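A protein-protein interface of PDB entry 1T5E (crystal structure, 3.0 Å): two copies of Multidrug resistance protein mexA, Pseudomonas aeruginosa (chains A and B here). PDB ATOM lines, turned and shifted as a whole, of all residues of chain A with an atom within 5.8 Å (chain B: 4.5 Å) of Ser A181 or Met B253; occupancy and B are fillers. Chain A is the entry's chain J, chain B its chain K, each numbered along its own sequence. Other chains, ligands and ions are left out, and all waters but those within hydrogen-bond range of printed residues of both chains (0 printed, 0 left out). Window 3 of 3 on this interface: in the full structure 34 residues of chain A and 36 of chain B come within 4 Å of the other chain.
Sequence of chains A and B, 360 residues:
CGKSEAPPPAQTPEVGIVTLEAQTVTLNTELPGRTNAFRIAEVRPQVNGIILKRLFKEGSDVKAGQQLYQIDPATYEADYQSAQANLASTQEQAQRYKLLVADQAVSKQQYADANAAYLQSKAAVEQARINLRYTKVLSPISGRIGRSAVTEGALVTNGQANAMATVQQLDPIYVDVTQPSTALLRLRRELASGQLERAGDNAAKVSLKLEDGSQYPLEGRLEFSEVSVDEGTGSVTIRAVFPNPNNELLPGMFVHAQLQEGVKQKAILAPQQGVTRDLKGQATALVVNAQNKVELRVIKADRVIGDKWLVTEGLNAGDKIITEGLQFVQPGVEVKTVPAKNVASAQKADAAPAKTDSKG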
ATOM      1  N   GLN A 179     -20.804  -2.791  13.513  1.00  0.00           N
ATOM      2  CA  GLN A 179     -20.819  -1.574  14.329  1.00  0.00           C
ATOM      3  C   GLN A 179     -19.581  -1.516  15.221  1.00  0.00           C
ATOM      4  O   GLN A 179     -19.032  -2.560  15.585  1.00  0.00           O
ATOM      5  CB  GLN A 179     -22.062  -1.557  15.235  1.00  0.00           C
ATOM      6  CG  GLN A 179     -23.372  -1.292  14.522  1.00  0.00           C
ATOM      7  CD  GLN A 179     -23.431   0.097  13.891  1.00  0.00           C
ATOM      8  OE1 GLN A 179     -23.493   1.107  14.590  1.00  0.00           O
ATOM      9  NE2 GLN A 179     -23.402   0.149  12.561  1.00  0.00           N
ATOM     10  N   PRO A 180     -19.116  -0.297  15.573  1.00  0.00           N
ATOM     11  CA  PRO A 180     -17.937  -0.162  16.441  1.00  0.00           C
ATOM     12  C   PRO A 180     -18.320  -0.691  17.822  1.00  0.00           C
ATOM     13  O   PRO A 180     -19.394  -0.370  18.335  1.00  0.00           O
ATOM     14  CB  PRO A 180     -17.683   1.341  16.453  1.00  0.00           C
ATOM     15  CG  PRO A 180     -18.168   1.765  15.103  1.00  0.00           C
ATOM     16  CD  PRO A 180     -19.470   1.006  14.983  1.00  0.00           C
ATOM     17  N   SER A 181     -17.448  -1.504  18.407  1.00  0.00           N
ATOM     18  CA  SER A 181     -17.694  -2.119  19.706  1.00  0.00           C
ATOM     19  C   SER A 181     -18.510  -1.267  20.679  1.00  0.00           C
ATOM     20  O   SER A 181     -19.314  -1.789  21.450  1.00  0.00           O
ATOM     21  CB  SER A 181     -16.363  -2.503  20.347  1.00  0.00           C
ATOM     22  OG  SER A 181     -16.583  -3.342  21.462  1.00  0.00           O
ATOM     23  N   THR A 182     -18.295   0.042  20.641  1.00  0.00           N
ATOM     24  CA  THR A 182     -19.011   0.975  21.506  1.00  0.00           C
ATOM     25  C   THR A 182     -20.510   0.913  21.250  1.00  0.00           C
ATOM     26  O   THR A 182     -21.308   0.651  22.159  1.00  0.00           O
ATOM     27  CB  THR A 182     -18.565   2.405  21.230  1.00  0.00           C
ATOM     28  OG1 THR A 182     -17.172   2.535  21.533  1.00  0.00           O
ATOM     29  CG2 THR A 182     -19.391   3.386  22.060  1.00  0.00           C
ATOM     30  N   ALA A 183     -20.872   1.182  19.995  1.00  0.00           N
ATOM     31  CA  ALA A 183     -22.254   1.180  19.542  1.00  0.00           C
ATOM     32  C   ALA A 183     -22.984  -0.097  19.936  1.00  0.00           C
ATOM     33  O   ALA A 183     -24.138  -0.047  20.359  1.00  0.00           O
ATOM     34  CB  ALA A 183     -22.293   1.358  18.039  1.00  0.00           C
ATOM     35  N   LEU A 184     -22.316  -1.237  19.799  1.00  0.00           N
ATOM     36  CA  LEU A 184     -22.929  -2.511  20.144  1.00  0.00           C
ATOM     37  C   LEU A 184     -23.394  -2.492  21.600  1.00  0.00           C
ATOM     38  O   LEU A 184     -24.426  -3.074  21.931  1.00  0.00           O
ATOM     39  CB  LEU A 184     -21.944  -3.663  19.893  1.00  0.00           C
ATOM     40  CG  LEU A 184     -22.415  -5.118  19.993  1.00  0.00           C
ATOM     41  CD1 LEU A 184     -22.417  -5.603  21.426  1.00  0.00           C
ATOM     42  CD2 LEU A 184     -23.795  -5.232  19.406  1.00  0.00           C
ATOM     43  N   LEU A 185     -22.643  -1.817  22.469  1.00  0.00           N
ATOM     44  CA  LEU A 185     -23.020  -1.729  23.882  1.00  0.00           C
ATOM     45  C   LEU A 185     -24.195  -0.778  24.033  1.00  0.00           C
ATOM     46  O   LEU A 185     -25.200  -1.100  24.686  1.00  0.00           O
ATOM     47  CB  LEU A 185     -21.855  -1.219  24.733  1.00  0.00           C
ATOM     48  CG  LEU A 185     -20.849  -2.264  25.207  1.00  0.00           C
ATOM     49  CD1 LEU A 185     -19.756  -1.564  25.998  1.00  0.00           C
ATOM     50  CD2 LEU A 185     -21.544  -3.324  26.067  1.00  0.00           C
ATOM     51  N   ARG A 186     -24.053   0.398  23.425  1.00  0.00           N
ATOM     52  CA  ARG A 186     -25.092   1.418  23.456  1.00  0.00           C
ATOM     53  C   ARG A 186     -26.451   0.779  23.129  1.00  0.00           C
ATOM     54  O   ARG A 186     -27.427   0.940  23.870  1.00  0.00           O
ATOM     55  CB  ARG A 186     -24.740   2.523  22.451  1.00  0.00           C
ATOM     56  CG  ARG A 186     -25.675   3.724  22.457  1.00  0.00           C
ATOM     57  CD  ARG A 186     -26.950   3.454  21.671  1.00  0.00           C
ATOM     58  NE  ARG A 186     -27.006   4.173  20.394  1.00  0.00           N
ATOM     59  CZ  ARG A 186     -26.072   4.120  19.442  1.00  0.00           C
ATOM     60  NH1 ARG A 186     -24.976   3.384  19.601  1.00  0.00           N
ATOM     61  NH2 ARG A 186     -26.248   4.794  18.310  1.00  0.00           N
ATOM     62  N   GLU A 231     -10.233  -7.410  15.534  1.00  0.00           N
ATOM     63  CA  GLU A 231      -9.371  -6.807  16.551  1.00  0.00           C
ATOM     64  C   GLU A 231      -8.471  -5.691  16.021  1.00  0.00           C
ATOM     65  O   GLU A 231      -8.017  -4.834  16.779  1.00  0.00           O
ATOM     66  CB  GLU A 231      -8.547  -7.898  17.233  1.00  0.00           C
ATOM     67  CG  GLU A 231      -9.436  -8.896  17.956  1.00  0.00           C
ATOM     68  CD  GLU A 231      -8.668  -9.965  18.717  1.00  0.00           C
ATOM     69  OE1 GLU A 231      -7.725  -9.617  19.470  1.00  0.00           O
ATOM     70  OE2 GLU A 231      -9.023 -11.160  18.581  1.00  0.00           O
ATOM     71  N   GLY A 234     -11.327  -3.281  15.987  1.00  0.00           N
ATOM     72  CA  GLY A 234     -12.076  -3.280  17.232  1.00  0.00           C
ATOM     73  C   GLY A 234     -13.574  -3.445  17.008  1.00  0.00           C
ATOM     74  O   GLY A 234     -14.320  -3.758  17.949  1.00  0.00           O
ATOM     75  N   SER A 235     -14.006  -3.241  15.757  1.00  0.00           N
ATOM     76  CA  SER A 235     -15.416  -3.344  15.360  1.00  0.00           C
ATOM     77  C   SER A 235     -15.973  -4.761  15.445  1.00  0.00           C
ATOM     78  O   SER A 235     -15.284  -5.736  15.144  1.00  0.00           O
ATOM     79  CB  SER A 235     -15.608  -2.822  13.938  1.00  0.00           C
ATOM     80  OG  SER A 235     -14.894  -3.626  13.025  1.00  0.00           O
ATOM     81  N   VAL A 236     -17.239  -4.851  15.848  1.00  0.00           N
ATOM     82  CA  VAL A 236     -17.923  -6.131  16.009  1.00  0.00           C
ATOM     83  C   VAL A 236     -18.858  -6.374  14.847  1.00  0.00           C
ATOM     84  O   VAL A 236     -19.227  -5.446  14.129  1.00  0.00           O
ATOM     85  CB  VAL A 236     -18.771  -6.159  17.300  1.00  0.00           C
ATOM     86  CG1 VAL A 236     -19.152  -7.588  17.655  1.00  0.00           C
ATOM     87  CG2 VAL A 236     -18.013  -5.506  18.426  1.00  0.00           C
ATOM     88  N   GLY B  33      -4.486   1.607  26.305  1.00  0.00           N
ATOM     89  CA  GLY B  33      -4.271   0.202  25.992  1.00  0.00           C
ATOM     90  C   GLY B  33      -5.304  -0.405  25.054  1.00  0.00           C
ATOM     91  O   GLY B  33      -6.263   0.254  24.670  1.00  0.00           O
ATOM     92  N   ARG B  34      -5.100  -1.665  24.682  1.00  0.00           N
ATOM     93  CA  ARG B  34      -6.001  -2.385  23.794  1.00  0.00           C
ATOM     94  C   ARG B  34      -6.498  -3.618  24.512  1.00  0.00           C
ATOM     95  O   ARG B  34      -5.766  -4.240  25.257  1.00  0.00           O
ATOM     96  CB  ARG B  34      -5.270  -2.826  22.536  1.00  0.00           C
ATOM     97  CG  ARG B  34      -4.716  -1.690  21.705  1.00  0.00           C
ATOM     98  CD  ARG B  34      -5.836  -0.833  21.142  1.00  0.00           C
ATOM     99  NE  ARG B  34      -5.961  -0.934  19.688  1.00  0.00           N
ATOM    100  CZ  ARG B  34      -6.156  -2.071  19.028  1.00  0.00           C
ATOM    101  NH1 ARG B  34      -6.241  -3.219  19.690  1.00  0.00           N
ATOM    102  NH2 ARG B  34      -6.291  -2.058  17.706  1.00  0.00           N
ATOM    103  N   THR B  35      -7.750  -3.977  24.302  1.00  0.00           N
ATOM    104  CA  THR B  35      -8.290  -5.169  24.945  1.00  0.00           C
ATOM    105  C   THR B  35      -7.848  -6.381  24.129  1.00  0.00           C
ATOM    106  O   THR B  35      -7.710  -6.290  22.911  1.00  0.00           O
ATOM    107  CB  THR B  35      -9.837  -5.115  24.991  1.00  0.00           C
ATOM    108  OG1 THR B  35     -10.328  -4.581  23.752  1.00  0.00           O
ATOM    109  CG2 THR B  35     -10.309  -4.236  26.133  1.00  0.00           C
ATOM    110  N   LEU B 210     -13.812   3.120  28.473  1.00  0.00           N
ATOM    111  CA  LEU B 210     -13.981   2.820  27.048  1.00  0.00           C
ATOM    112  C   LEU B 210     -13.752   4.054  26.184  1.00  0.00           C
ATOM    113  O   LEU B 210     -13.954   5.176  26.646  1.00  0.00           O
ATOM    114  CB  LEU B 210     -15.387   2.281  26.811  1.00  0.00           C
ATOM    115  CG  LEU B 210     -15.910   1.354  27.911  1.00  0.00           C
ATOM    116  CD1 LEU B 210     -17.310   0.878  27.578  1.00  0.00           C
ATOM    117  CD2 LEU B 210     -14.982   0.175  28.066  1.00  0.00           C
ATOM    118  N   GLU B 211     -13.330   3.855  24.935  1.00  0.00           N
ATOM    119  CA  GLU B 211     -13.080   4.984  24.029  1.00  0.00           C
ATOM    120  C   GLU B 211     -14.386   5.707  23.809  1.00  0.00           C
ATOM    121  O   GLU B 211     -14.456   6.748  23.166  1.00  0.00           O
ATOM    122  CB  GLU B 211     -12.518   4.510  22.687  1.00  0.00           C
ATOM    123  CG  GLU B 211     -13.377   3.501  21.951  1.00  0.00           C
ATOM    124  CD  GLU B 211     -12.775   3.104  20.605  1.00  0.00           C
ATOM    125  OE1 GLU B 211     -12.601   3.999  19.740  1.00  0.00           O
ATOM    126  OE2 GLU B 211     -12.473   1.901  20.411  1.00  0.00           O
ATOM    127  N   LEU B 249     -17.215  -6.406  26.923  1.00  0.00           N
ATOM    128  CA  LEU B 249     -15.900  -6.070  26.379  1.00  0.00           C
ATOM    129  C   LEU B 249     -15.435  -7.015  25.283  1.00  0.00           C
ATOM    130  O   LEU B 249     -15.525  -8.234  25.426  1.00  0.00           O
ATOM    131  CB  LEU B 249     -14.883  -6.061  27.516  1.00  0.00           C
ATOM    132  CG  LEU B 249     -15.096  -4.936  28.526  1.00  0.00           C
ATOM    133  CD1 LEU B 249     -14.199  -5.147  29.719  1.00  0.00           C
ATOM    134  CD2 LEU B 249     -14.820  -3.595  27.853  1.00  0.00           C
ATOM    135  N   LEU B 250     -14.926  -6.457  24.191  1.00  0.00           N
ATOM    136  CA  LEU B 250     -14.457  -7.292  23.093  1.00  0.00           C
ATOM    137  C   LEU B 250     -13.056  -6.911  22.648  1.00  0.00           C
ATOM    138  O   LEU B 250     -12.655  -5.761  22.758  1.00  0.00           O
ATOM    139  CB  LEU B 250     -15.409  -7.186  21.900  1.00  0.00           C
ATOM    140  CG  LEU B 250     -16.842  -7.698  22.094  1.00  0.00           C
ATOM    141  CD1 LEU B 250     -17.592  -7.476  20.808  1.00  0.00           C
ATOM    142  CD2 LEU B 250     -16.864  -9.173  22.476  1.00  0.00           C
ATOM    143  N   PRO B 251     -12.292  -7.878  22.127  1.00  0.00           N
ATOM    144  CA  PRO B 251     -10.926  -7.633  21.661  1.00  0.00           C
ATOM    145  C   PRO B 251     -10.824  -6.505  20.645  1.00  0.00           C
ATOM    146  O   PRO B 251     -11.710  -6.342  19.814  1.00  0.00           O
ATOM    147  CB  PRO B 251     -10.532  -8.969  21.056  1.00  0.00           C
ATOM    148  CG  PRO B 251     -11.275  -9.953  21.899  1.00  0.00           C
ATOM    149  CD  PRO B 251     -12.632  -9.308  22.030  1.00  0.00           C
ATOM    150  N   GLY B 252      -9.750  -5.721  20.721  1.00  0.00           N
ATOM    151  CA  GLY B 252      -9.544  -4.644  19.765  1.00  0.00           C
ATOM    152  C   GLY B 252      -9.999  -3.262  20.174  1.00  0.00           C
ATOM    153  O   GLY B 252      -9.737  -2.288  19.458  1.00  0.00           O
ATOM    154  N   MET B 253     -10.680  -3.164  21.316  1.00  0.00           N
ATOM    155  CA  MET B 253     -11.172  -1.873  21.800  1.00  0.00           C
ATOM    156  C   MET B 253      -9.998  -1.031  22.261  1.00  0.00           C
ATOM    157  O   MET B 253      -9.051  -1.554  22.837  1.00  0.00           O
ATOM    158  CB  MET B 253     -12.143  -2.064  22.977  1.00  0.00           C
ATOM    159  CG  MET B 253     -13.399  -2.863  22.661  1.00  0.00           C
ATOM    160  SD  MET B 253     -14.483  -3.124  24.103  1.00  0.00           S
ATOM    161  CE  MET B 253     -15.276  -1.510  24.135  1.00  0.00           C
ATOM    162  N   PHE B 254     -10.049   0.268  21.995  1.00  0.00           N
ATOM    163  CA  PHE B 254      -8.993   1.175  22.435  1.00  0.00           C
ATOM    164  C   PHE B 254      -9.492   1.805  23.729  1.00  0.00           C
ATOM    165  O   PHE B 254     -10.296   2.727  23.696  1.00  0.00           O
ATOM    166  CB  PHE B 254      -8.742   2.275  21.399  1.00  0.00           C
ATOM    167  CG  PHE B 254      -8.200   1.767  20.082  1.00  0.00           C
ATOM    168  CD1 PHE B 254      -8.947   0.887  19.291  1.00  0.00           C
ATOM    169  CD2 PHE B 254      -6.942   2.173  19.626  1.00  0.00           C
ATOM    170  CE1 PHE B 254      -8.447   0.420  18.063  1.00  0.00           C
ATOM    171  CE2 PHE B 254      -6.434   1.714  18.405  1.00  0.00           C
ATOM    172  CZ  PHE B 254      -7.187   0.836  17.624  1.00  0.00           C
ATOM    173  N   VAL B 255      -9.014   1.311  24.866  1.00  0.00           N
ATOM    174  CA  VAL B 255      -9.447   1.822  26.159  1.00  0.00           C
ATOM    175  C   VAL B 255      -8.390   2.592  26.956  1.00  0.00           C
ATOM    176  O   VAL B 255      -7.322   2.928  26.438  1.00  0.00           O
ATOM    177  CB  VAL B 255      -9.966   0.669  27.018  1.00  0.00           C
ATOM    178  CG1 VAL B 255     -11.123   0.002  26.314  1.00  0.00           C
ATOM    179  CG2 VAL B 255      -8.857  -0.337  27.259  1.00  0.00           C
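Of the printed residues of chain B, Ser A181 touches Met B253.
Met B253 touches just one residue of chain A: Ser A181 (3.4 Å).
Printed residues of chain B within 4 Å of Val A236: Leu B250 (3.1 Å).
Printed residues of chain A within 4 Å of Leu B250: Val A236 (3.1 Å).
The nearest residue of chain B that does not touch Ser A181 is Leu B250 (4.04 Å).
The nearest residue of chain A that does not touch Met B253 is Gly A234 (4.3 Å).
The nearest printed residue of chain B that does not touch Glu A231 is Thr B35 (4.8 Å).
OG1 of Thr A182 touches CG of Glu B211 (3.9 Å).
Leu B210 touches Leu A185 (CD1 to CD1, 3.8 Å).
Pro B251 touches Glu A231 (CB to CD, 3.2 Å).
Glu A231 touches Gly B252 (O to CA, 3.4 Å).
CA of Gly A234 touches O of Gly B252, at 3.4 Å.
CG2 of Val A236 touches CD1 of Leu B250, at 3.1 Å.
The side-chain carboxylate of Glu B211 is in hydrogen-bond range of the backbone NH of Phe B254 (3.3 Å).
The backbone carbonyl oxygen of Gln A179 is in hydrogen-bond range of the backbone NH of Val A236, at 2.9 Å.
The backbone NH (N) of Leu B250 sits at hydrogen-bond distance from the side-chain sulfur (SD) of Met B253 (3.4 Å).
The side-chain hydroxyl of Thr B35 sits at hydrogen-bond distance from the backbone carbonyl oxygen of Leu B250 (2.8 Å).
O of Thr B35 lies within hydrogen-bond range of N of Gly B252 (3.0 Å).
The side-chain hydroxyl of Thr B35 sits at hydrogen-bond distance from the backbone NH of Met B253 (2.8 Å).
NH2 of Arg B34 lies within hydrogen-bond range of O of Glu A231 (3.4 Å).
SD of Met B253 lies within hydrogen-bond range of OG of Ser A181 (3.4 Å).
Hydrophobic or aromatic side chains of chain B within 4 Å of the printed part of chain A: Leu B210, Leu B250, Pro B251 and Met B253.
Along chain B the printed residues that touch a printed residue of chain A span positions 34 to 253.
Of the 12 printed residues of chain A, 6 touch a printed residue of chain B.
Among the printed residues, 8 pairs touch across the chains.
No position is printed for both chains.
Of the 8 pairs that touch across the chains among the printed residues, none has its exchanged pair printed and touching as well.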
